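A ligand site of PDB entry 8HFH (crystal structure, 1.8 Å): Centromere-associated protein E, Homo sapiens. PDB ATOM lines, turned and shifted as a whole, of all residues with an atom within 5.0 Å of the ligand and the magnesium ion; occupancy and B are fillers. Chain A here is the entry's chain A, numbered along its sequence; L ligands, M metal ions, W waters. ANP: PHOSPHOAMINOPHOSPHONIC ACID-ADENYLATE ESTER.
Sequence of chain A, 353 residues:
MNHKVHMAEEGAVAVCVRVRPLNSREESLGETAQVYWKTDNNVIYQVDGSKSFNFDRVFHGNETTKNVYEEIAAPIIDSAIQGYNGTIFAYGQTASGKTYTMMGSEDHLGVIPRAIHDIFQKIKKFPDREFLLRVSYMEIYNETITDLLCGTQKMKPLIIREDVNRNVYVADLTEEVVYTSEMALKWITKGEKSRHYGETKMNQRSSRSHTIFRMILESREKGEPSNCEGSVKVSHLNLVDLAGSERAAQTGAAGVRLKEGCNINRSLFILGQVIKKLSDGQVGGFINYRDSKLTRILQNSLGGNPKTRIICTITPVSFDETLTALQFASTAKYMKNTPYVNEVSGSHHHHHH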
ATOM      1  N   ARG A  18      -8.033 -27.296  -9.326  1.00  0.00           N
ATOM      2  CA  ARG A  18      -7.044 -28.395  -9.280  1.00  0.00           C
ATOM      3  C   ARG A  18      -5.679 -27.794  -9.521  1.00  0.00           C
ATOM      4  O   ARG A  18      -5.453 -27.259 -10.601  1.00  0.00           O
ATOM      5  CB  ARG A  18      -7.371 -29.500 -10.279  1.00  0.00           C
ATOM      6  CG  ARG A  18      -6.366 -30.642 -10.177  1.00  0.00           C
ATOM      7  CD  ARG A  18      -6.637 -31.770 -11.135  1.00  0.00           C
ATOM      8  NE  ARG A  18      -5.925 -32.948 -10.681  1.00  0.00           N
ATOM      9  CZ  ARG A  18      -5.964 -34.139 -11.269  1.00  0.00           C
ATOM     10  NH1 ARG A  18      -6.674 -34.326 -12.367  1.00  0.00           N
ATOM     11  NH2 ARG A  18      -5.337 -35.177 -10.725  1.00  0.00           N
ATOM     12  N   ARG A  20      -1.864 -28.620 -10.188  1.00  0.00           N
ATOM     13  CA  ARG A  20      -1.003 -29.730 -10.595  1.00  0.00           C
ATOM     14  C   ARG A  20       0.381 -29.567  -9.963  1.00  0.00           C
ATOM     15  O   ARG A  20       0.839 -28.466  -9.611  1.00  0.00           O
ATOM     16  CB  ARG A  20      -0.875 -29.785 -12.113  1.00  0.00           C
ATOM     17  CG  ARG A  20      -0.369 -28.512 -12.778  1.00  0.00           C
ATOM     18  CD  ARG A  20       0.071 -28.906 -14.203  1.00  0.00           C
ATOM     19  NE  ARG A  20       0.569 -27.843 -15.031  1.00  0.00           N
ATOM     20  CZ  ARG A  20       1.775 -27.255 -14.940  1.00  0.00           C
ATOM     21  NH1 ARG A  20       2.627 -27.600 -13.979  1.00  0.00           N
ATOM     22  NH2 ARG A  20       2.074 -26.258 -15.756  1.00  0.00           N
ATOM     23  N   PRO A  21       1.175 -30.659  -9.999  1.00  0.00           N
ATOM     24  CA  PRO A  21       2.594 -30.583  -9.697  1.00  0.00           C
ATOM     25  C   PRO A  21       3.306 -29.833 -10.826  1.00  0.00           C
ATOM     26  O   PRO A  21       2.759 -29.766 -11.909  1.00  0.00           O
ATOM     27  CB  PRO A  21       3.086 -32.034  -9.656  1.00  0.00           C
ATOM     28  CG  PRO A  21       1.840 -32.879  -9.695  1.00  0.00           C
ATOM     29  CD  PRO A  21       0.762 -32.024 -10.375  1.00  0.00           C
ATOM     30  N   GLY A  61      -1.603 -31.173  -5.673  1.00  0.00           N
ATOM     31  CA  GLY A  61      -0.786 -31.869  -6.694  1.00  0.00           C
ATOM     32  C   GLY A  61      -0.720 -33.365  -6.502  1.00  0.00           C
ATOM     33  O   GLY A  61      -0.535 -34.042  -7.558  1.00  0.00           O
ATOM     34  N   GLY A  92      -8.615 -23.277 -17.747  1.00  0.00           N
ATOM     35  CA  GLY A  92      -7.301 -22.878 -17.236  1.00  0.00           C
ATOM     36  C   GLY A  92      -6.289 -22.645 -18.331  1.00  0.00           C
ATOM     37  O   GLY A  92      -6.528 -23.010 -19.490  1.00  0.00           O
ATOM     38  N   GLN A  93      -5.174 -22.022 -17.949  1.00  0.00           N
ATOM     39  CA  GLN A  93      -4.054 -21.697 -18.867  1.00  0.00           C
ATOM     40  C   GLN A  93      -3.614 -22.948 -19.645  1.00  0.00           C
ATOM     41  O   GLN A  93      -3.754 -24.100 -19.168  1.00  0.00           O
ATOM     42  CB  GLN A  93      -2.951 -21.200 -17.936  1.00  0.00           C
ATOM     43  CG  GLN A  93      -1.673 -20.921 -18.608  1.00  0.00           C
ATOM     44  CD  GLN A  93      -0.545 -20.677 -17.650  1.00  0.00           C
ATOM     45  OE1 GLN A  93      -0.517 -21.060 -16.470  1.00  0.00           O
ATOM     46  NE2 GLN A  93       0.414 -19.998 -18.209  1.00  0.00           N
ATOM     47  N   THR A  94      -2.987 -22.747 -20.806  1.00  0.00           N
ATOM     48  CA  THR A  94      -2.307 -23.859 -21.516  1.00  0.00           C
ATOM     49  C   THR A  94      -1.377 -24.591 -20.519  1.00  0.00           C
ATOM     50  O   THR A  94      -0.652 -23.936 -19.684  1.00  0.00           O
ATOM     51  CB  THR A  94      -1.591 -23.347 -22.780  1.00  0.00           C
ATOM     52  OG1 THR A  94      -1.057 -24.484 -23.440  1.00  0.00           O
ATOM     53  CG2 THR A  94      -0.467 -22.394 -22.455  1.00  0.00           C
ATOM     54  N   ALA A  95      -1.420 -25.918 -20.588  1.00  0.00           N
ATOM     55  CA  ALA A  95      -0.545 -26.884 -19.871  1.00  0.00           C
ATOM     56  C   ALA A  95      -0.884 -26.939 -18.376  1.00  0.00           C
ATOM     57  O   ALA A  95      -0.099 -27.548 -17.597  1.00  0.00           O
ATOM     58  CB  ALA A  95       0.909 -26.535 -20.082  1.00  0.00           C
ATOM     59  N   SER A  96      -2.034 -26.392 -17.984  1.00  0.00           N
ATOM     60  CA  SER A  96      -2.459 -26.359 -16.576  1.00  0.00           C
ATOM     61  C   SER A  96      -3.067 -27.709 -16.146  1.00  0.00           C
ATOM     62  O   SER A  96      -3.041 -27.992 -14.915  1.00  0.00           O
ATOM     63  CB  SER A  96      -3.412 -25.184 -16.299  1.00  0.00           C
ATOM     64  OG  SER A  96      -4.630 -25.291 -17.026  1.00  0.00           O
ATOM     65  N   GLY A  97      -3.591 -28.532 -17.068  1.00  0.00           N
ATOM     66  CA  GLY A  97      -4.102 -29.880 -16.723  1.00  0.00           C
ATOM     67  C   GLY A  97      -5.527 -30.191 -17.161  1.00  0.00           C
ATOM     68  O   GLY A  97      -6.125 -31.127 -16.607  1.00  0.00           O
ATOM     69  N   LYS A  98      -6.134 -29.385 -18.019  1.00  0.00           N
ATOM     70  CA  LYS A  98      -7.538 -29.628 -18.459  1.00  0.00           C
ATOM     71  C   LYS A  98      -7.685 -31.006 -19.143  1.00  0.00           C
ATOM     72  O   LYS A  98      -8.609 -31.731 -18.809  1.00  0.00           O
ATOM     73  CB  LYS A  98      -7.969 -28.536 -19.429  1.00  0.00           C
ATOM     74  CG  LYS A  98      -7.938 -27.104 -18.897  1.00  0.00           C
ATOM     75  CD  LYS A  98      -8.324 -26.072 -19.921  1.00  0.00           C
ATOM     76  CE  LYS A  98      -7.293 -25.915 -21.043  1.00  0.00           C
ATOM     77  NZ  LYS A  98      -5.945 -25.546 -20.553  1.00  0.00           N
ATOM     78  N   THR A  99      -6.843 -31.314 -20.123  1.00  0.00           N
ATOM     79  CA  THR A  99      -6.974 -32.580 -20.895  1.00  0.00           C
ATOM     80  C   THR A  99      -6.565 -33.752 -19.995  1.00  0.00           C
ATOM     81  O   THR A  99      -7.181 -34.836 -20.093  1.00  0.00           O
ATOM     82  CB  THR A  99      -6.231 -32.459 -22.209  1.00  0.00           C
ATOM     83  OG1 THR A  99      -6.740 -31.323 -22.917  1.00  0.00           O
ATOM     84  CG2 THR A  99      -6.430 -33.683 -23.082  1.00  0.00           C
ATOM     85  N   TYR A 100      -5.498 -33.591 -19.242  1.00  0.00           N
ATOM     86  CA  TYR A 100      -5.063 -34.565 -18.209  1.00  0.00           C
ATOM     87  C   TYR A 100      -6.296 -34.922 -17.361  1.00  0.00           C
ATOM     88  O   TYR A 100      -6.598 -36.079 -17.125  1.00  0.00           O
ATOM     89  CB  TYR A 100      -3.887 -34.012 -17.408  1.00  0.00           C
ATOM     90  CG  TYR A 100      -3.431 -34.947 -16.320  1.00  0.00           C
ATOM     91  CD1 TYR A 100      -4.038 -34.942 -15.086  1.00  0.00           C
ATOM     92  CD2 TYR A 100      -2.473 -35.936 -16.577  1.00  0.00           C
ATOM     93  CE1 TYR A 100      -3.620 -35.803 -14.073  1.00  0.00           C
ATOM     94  CE2 TYR A 100      -2.067 -36.803 -15.575  1.00  0.00           C
ATOM     95  CZ  TYR A 100      -2.650 -36.753 -14.335  1.00  0.00           C
ATOM     96  OH  TYR A 100      -2.245 -37.627 -13.365  1.00  0.00           O
ATOM     97  N   THR A 101      -7.002 -33.912 -16.865  1.00  0.00           N
ATOM     98  CA  THR A 101      -8.173 -34.103 -15.977  1.00  0.00           C
ATOM     99  C   THR A 101      -9.384 -34.693 -16.733  1.00  0.00           C
ATOM    100  O   THR A 101     -10.012 -35.628 -16.202  1.00  0.00           O
ATOM    101  CB  THR A 101      -8.512 -32.801 -15.258  1.00  0.00           C
ATOM    102  OG1 THR A 101      -7.366 -32.448 -14.470  1.00  0.00           O
ATOM    103  CG2 THR A 101      -9.742 -32.909 -14.385  1.00  0.00           C
ATOM    104  N   ARG A 195      -9.456 -34.727 -33.668  1.00  0.00           N
ATOM    105  CA  ARG A 195      -9.327 -33.526 -32.782  1.00  0.00           C
ATOM    106  C   ARG A 195      -8.042 -32.752 -33.120  1.00  0.00           C
ATOM    107  O   ARG A 195      -6.990 -33.365 -33.333  1.00  0.00           O
ATOM    108  CB  ARG A 195      -9.409 -34.003 -31.335  1.00  0.00           C
ATOM    109  CG  ARG A 195      -9.144 -32.924 -30.302  1.00  0.00           C
ATOM    110  CD  ARG A 195      -9.368 -33.495 -28.934  1.00  0.00           C
ATOM    111  NE  ARG A 195      -9.097 -32.468 -27.926  1.00  0.00           N
ATOM    112  CZ  ARG A 195      -9.141 -32.665 -26.620  1.00  0.00           C
ATOM    113  NH1 ARG A 195      -8.830 -31.659 -25.803  1.00  0.00           N
ATOM    114  NH2 ARG A 195      -9.502 -33.855 -26.139  1.00  0.00           N
ATOM    115  N   ASN A 203       3.145 -26.679 -24.296  1.00  0.00           N
ATOM    116  CA  ASN A 203       2.481 -28.011 -24.311  1.00  0.00           C
ATOM    117  C   ASN A 203       2.809 -28.722 -25.614  1.00  0.00           C
ATOM    118  O   ASN A 203       2.442 -28.240 -26.674  1.00  0.00           O
ATOM    119  CB  ASN A 203       0.982 -27.859 -24.031  1.00  0.00           C
ATOM    120  CG  ASN A 203       0.313 -29.178 -23.703  1.00  0.00           C
ATOM    121  OD1 ASN A 203       0.832 -30.268 -24.016  1.00  0.00           O
ATOM    122  ND2 ASN A 203      -0.839 -29.123 -23.070  1.00  0.00           N
ATOM    123  N   ARG A 205       1.360 -31.191 -26.689  1.00  0.00           N
ATOM    124  CA  ARG A 205       0.051 -31.642 -27.215  1.00  0.00           C
ATOM    125  C   ARG A 205      -1.056 -30.739 -26.653  1.00  0.00           C
ATOM    126  O   ARG A 205      -1.964 -31.205 -25.898  1.00  0.00           O
ATOM    127  CB  ARG A 205      -0.151 -33.114 -26.895  1.00  0.00           C
ATOM    128  CG  ARG A 205      -1.151 -33.782 -27.808  1.00  0.00           C
ATOM    129  CD  ARG A 205      -0.710 -35.237 -27.861  1.00  0.00           C
ATOM    130  NE  ARG A 205      -1.842 -36.083 -27.834  1.00  0.00           N
ATOM    131  CZ  ARG A 205      -2.621 -36.352 -28.854  1.00  0.00           C
ATOM    132  NH1 ARG A 205      -2.352 -35.859 -30.046  1.00  0.00           N
ATOM    133  NH2 ARG A 205      -3.624 -37.174 -28.655  1.00  0.00           N
ATOM    134  N   SER A 206      -0.955 -29.469 -27.050  1.00  0.00           N
ATOM    135  CA  SER A 206      -1.924 -28.410 -26.735  1.00  0.00           C
ATOM    136  C   SER A 206      -3.214 -28.753 -27.501  1.00  0.00           C
ATOM    137  O   SER A 206      -3.155 -28.977 -28.759  1.00  0.00           O
ATOM    138  CB  SER A 206      -1.446 -27.037 -27.110  1.00  0.00           C
ATOM    139  OG  SER A 206      -2.469 -26.119 -26.793  1.00  0.00           O
ATOM    140  N   SER A 207      -4.344 -28.658 -26.822  1.00  0.00           N
ATOM    141  CA  SER A 207      -5.705 -28.674 -27.417  1.00  0.00           C
ATOM    142  C   SER A 207      -5.971 -27.365 -28.164  1.00  0.00           C
ATOM    143  O   SER A 207      -6.081 -26.314 -27.518  1.00  0.00           O
ATOM    144  CB  SER A 207      -6.748 -28.872 -26.351  1.00  0.00           C
ATOM    145  OG  SER A 207      -6.405 -29.956 -25.486  1.00  0.00           O
ATOM    146  N   ASP A 241     -13.926 -29.907 -22.497  1.00  0.00           N
ATOM    147  CA  ASP A 241     -12.473 -29.629 -22.303  1.00  0.00           C
ATOM    148  C   ASP A 241     -12.137 -28.380 -23.121  1.00  0.00           C
ATOM    149  O   ASP A 241     -12.123 -28.443 -24.376  1.00  0.00           O
ATOM    150  CB  ASP A 241     -11.642 -30.836 -22.701  1.00  0.00           C
ATOM    151  CG  ASP A 241     -10.146 -30.654 -22.514  1.00  0.00           C
ATOM    152  OD1 ASP A 241      -9.716 -29.627 -21.990  1.00  0.00           O
ATOM    153  OD2 ASP A 241      -9.369 -31.598 -22.938  1.00  0.00           O
ATOM    154  N   LEU A 242     -11.992 -27.244 -22.432  1.00  0.00           N
ATOM    155  CA  LEU A 242     -11.762 -25.954 -23.151  1.00  0.00           C
ATOM    156  C   LEU A 242     -10.322 -25.908 -23.606  1.00  0.00           C
ATOM    157  O   LEU A 242      -9.468 -26.580 -23.001  1.00  0.00           O
ATOM    158  CB  LEU A 242     -12.088 -24.764 -22.232  1.00  0.00           C
ATOM    159  CG  LEU A 242     -13.510 -24.678 -21.692  1.00  0.00           C
ATOM    160  CD1 LEU A 242     -13.666 -23.449 -20.840  1.00  0.00           C
ATOM    161  CD2 LEU A 242     -14.504 -24.603 -22.840  1.00  0.00           C
ATOM    162  N   ALA A 243     -10.065 -25.134 -24.649  1.00  0.00           N
ATOM    163  CA  ALA A 243      -8.726 -24.591 -24.958  1.00  0.00           C
ATOM    164  C   ALA A 243      -8.334 -23.603 -23.856  1.00  0.00           C
ATOM    165  O   ALA A 243      -9.207 -23.238 -23.004  1.00  0.00           O
ATOM    166  CB  ALA A 243      -8.741 -23.979 -26.326  1.00  0.00           C
ATOM    167  N   GLY A 244      -7.040 -23.272 -23.776  1.00  0.00           N
ATOM    168  CA  GLY A 244      -6.474 -22.531 -22.630  1.00  0.00           C
ATOM    169  C   GLY A 244      -5.766 -21.264 -23.062  1.00  0.00           C
ATOM    170  O   GLY A 244      -5.268 -21.207 -24.185  1.00  0.00           O
ATOM    171  N   THR A 313      -8.134 -25.487 -13.576  1.00  0.00           N
ATOM    172  CA  THR A 313      -6.795 -26.091 -13.459  1.00  0.00           C
ATOM    173  C   THR A 313      -5.744 -24.957 -13.401  1.00  0.00           C
ATOM    174  O   THR A 313      -5.815 -24.038 -14.197  1.00  0.00           O
ATOM    175  CB  THR A 313      -6.574 -27.096 -14.587  1.00  0.00           C
ATOM    176  OG1 THR A 313      -6.862 -26.407 -15.812  1.00  0.00           O
ATOM    177  CG2 THR A 313      -7.424 -28.340 -14.423  1.00  0.00           C
HETATM  178  PG  ANP L   1      -3.841 -26.943 -23.383  1.00  0.00           P
HETATM  179  O1G ANP L   1      -4.702 -27.991 -24.116  1.00  0.00           O
HETATM  180  O2G ANP L   1      -2.654 -26.526 -24.177  1.00  0.00           O
HETATM  181  O3G ANP L   1      -4.728 -25.697 -23.166  1.00  0.00           O
HETATM  182  PB  ANP L   1      -4.047 -28.442 -20.922  1.00  0.00           P
HETATM  183  O1B ANP L   1      -4.526 -27.718 -19.687  1.00  0.00           O
HETATM  184  O2B ANP L   1      -5.003 -29.420 -21.552  1.00  0.00           O
HETATM  185  N3B ANP L   1      -3.377 -27.379 -21.911  1.00  0.00           N
HETATM  186  PA  ANP L   1      -2.706 -30.920 -20.283  1.00  0.00           P
HETATM  187  O1A ANP L   1      -3.891 -31.404 -19.546  1.00  0.00           O
HETATM  188  O2A ANP L   1      -2.421 -31.374 -21.693  1.00  0.00           O
HETATM  189  O3A ANP L   1      -2.829 -29.337 -20.439  1.00  0.00           O
HETATM  190  O5' ANP L   1      -1.352 -31.138 -19.390  1.00  0.00           O
HETATM  191  C5' ANP L   1      -0.002 -31.189 -19.951  1.00  0.00           C
HETATM  192  C4' ANP L   1       0.770 -32.252 -19.210  1.00  0.00           C
HETATM  193  O4' ANP L   1       0.903 -31.838 -17.840  1.00  0.00           O
HETATM  194  C3' ANP L   1       0.076 -33.602 -19.087  1.00  0.00           C
HETATM  195  O3' ANP L   1       0.261 -34.292 -20.296  1.00  0.00           O
HETATM  196  C2' ANP L   1       0.775 -34.215 -17.881  1.00  0.00           C
HETATM  197  O2' ANP L   1       2.099 -34.631 -18.148  1.00  0.00           O
HETATM  198  C1' ANP L   1       0.895 -32.978 -17.011  1.00  0.00           C
HETATM  199  N9  ANP L   1      -0.152 -32.859 -16.033  1.00  0.00           N
HETATM  200  C8  ANP L   1      -1.265 -32.056 -16.026  1.00  0.00           C
HETATM  201  N7  ANP L   1      -1.936 -32.132 -14.915  1.00  0.00           N
HETATM  202  C5  ANP L   1      -1.247 -33.087 -14.167  1.00  0.00           C
HETATM  203  C6  ANP L   1      -1.456 -33.620 -12.885  1.00  0.00           C
HETATM  204  N6  ANP L   1      -2.476 -33.263 -12.123  1.00  0.00           N
HETATM  205  N1  ANP L   1      -0.567 -34.567 -12.447  1.00  0.00           N
HETATM  206  C2  ANP L   1       0.463 -34.892 -13.236  1.00  0.00           C
HETATM  207  N3  ANP L   1       0.777 -34.421 -14.448  1.00  0.00           N
HETATM  208  C4  ANP L   1      -0.136 -33.514 -14.841  1.00  0.00           C
HETATM  209 MG    MG M   1      -5.670 -29.606 -23.453  1.00  0.00          MG
HETATM  210  O   HOH W   1       1.994 -29.167 -17.873  1.00  0.00           O
HETATM  211  O   HOH W   2      -1.253 -35.585  -9.954  1.00  0.00           O
HETATM  212  O   HOH W   3      -4.407 -31.540 -13.549  1.00  0.00           O
HETATM  213  O   HOH W   4       1.162 -32.853 -23.246  1.00  0.00           O
HETATM  214  O   HOH W   5      -7.552 -28.657 -23.133  1.00  0.00           O
HETATM  215  O   HOH W   6       2.599 -36.158 -15.759  1.00  0.00           O
HETATM  216  O   HOH W   7      -3.998 -30.869 -23.868  1.00  0.00           O
HETATM  217  O   HOH W   8      -5.320 -24.636 -25.558  1.00  0.00           O
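An oxygen (O1G) of the ligand sits close to the backbone NH (N) of Ser 207 (2.8 Å).
The backbone NH of Gly 244 lies within hydrogen-bond range of an oxygen (O3G) of the ligand, 3.4 Å away.
An oxygen (O1A) of the ligand lies within hydrogen-bond range of the backbone NH of Tyr 100, 2.7 Å away.
The backbone NH (N) of Lys 98 is in hydrogen-bond range of an oxygen (O1B) of the ligand.
An oxygen (O2A) of the ligand sits at hydrogen-bond distance from the side-chain amide nitrogen of Asn 203, at 3.1 Å.
The backbone NH of Ser 96 lies within hydrogen-bond range of an oxygen (O1B) of the ligand (3.3 Å).
OG1 of Thr 94 lies within hydrogen-bond range of O2G of the ligand.
O1B of the ligand is in salt-bridge range of NZ of Lys 98 (2.7 Å).
O2G of the ligand is in hydrogen-bond range of OG of Ser 206, 2.7 Å away.
An oxygen (O1A) of the ligand is in hydrogen-bond range of the backbone NH (N) of Thr 99 (3.0 Å).
O1B of the ligand lies within hydrogen-bond range of N of Gly 97, 2.9 Å away.
NZ of Lys 98 sits at hydrogen-bond distance from O of Gln 93, at 3.0 Å.
The side-chain hydroxyl (OG1) of Thr 101 is in hydrogen-bond range of the guanidinium group (NH1) of Arg 18 (2.9 Å).
NZ of Lys 98 sits at hydrogen-bond distance from O of Gly 92 (2.8 Å).
The backbone carbonyl oxygen of Gly 97 is in hydrogen-bond range of the side-chain hydroxyl of Thr 101, at 2.8 Å.
The side-chain hydroxyl of Thr 99 lies close to the side-chain carboxylate of Asp 241, at 2.6 Å.
The side-chain hydroxyl (OG) of Ser 96 lies within hydrogen-bond range of the side-chain hydroxyl (OG1) of Thr 313 (2.8 Å).
O of Ala 95 lies within hydrogen-bond range of NE of Arg 20.
The side-chain hydroxyl of Ser 207 sits close to the guanidinium group of Arg 195 (3.0 Å).
The backbone NH of Ala 95 lies close to a nitrogen (N3B) of the ligand (2.8 Å).
Merely in contact with the ligand: Arg 18, Arg 20, Pro 21 and Gln 93.
Hydrophobic or aromatic side chains within 4 Å of the ligand: Pro 21 and Tyr 100.
Within 4 Å of the ligand: Arg 18, Arg 20, Pro 21, Gln 93, Thr 94, Ala 95, Ser 96, Gly 97, Lys 98, Thr 99, Tyr 100, Asn 203, Ser 206, Ser 207 and Gly 244.
The nearest printed residue that does not touch the ligand is Ala 243 (4.2 Å).
Two residues have an atom within 4 Å of the magnesium ion: Thr 99 and Ser 207.
The nearest printed residue that does not touch the magnesium ion is Asp 241 (4.2 Å).
The magnesium ion is bound by an oxygen (O1G) of the ligand, an oxygen (O2B) of the ligand, the side-chain hydroxyl of Thr 99, water W5, water W7 and the side-chain hydroxyl of Ser 207.
The magnesium ion has six donor atoms within binding distance.
Water W7 lies within hydrogen-bond range of O2A of the ligand (2.7 Å) and O of Arg 205 (2.9 Å).
Water W5 bridges OD1 of Asp 241 (2.6 Å) and O of Leu 242 (2.8 Å).
Water W8 lies within hydrogen-bond range of O3G of the ligand (2.7 Å), O of Ser 207 (2.7 Å), N of Gly 244 (2.8 Å) and OG of Ser 206 (3.4 Å).
Water W2 lies within hydrogen-bond range of a nitrogen (N1) of the ligand (2.8 Å) and the backbone carbonyl oxygen of Gly 61 (2.9 Å).
Water W1 lies within hydrogen-bond range of the backbone carbonyl oxygen (O) of Ala 95, an oxygen (O4') of the ligand and the guanidinium group (NE) of Arg 20.
Water W3 bridges a nitrogen (N7) of the ligand (2.9 Å) and the side-chain hydroxyl of Thr 101 (3.2 Å).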
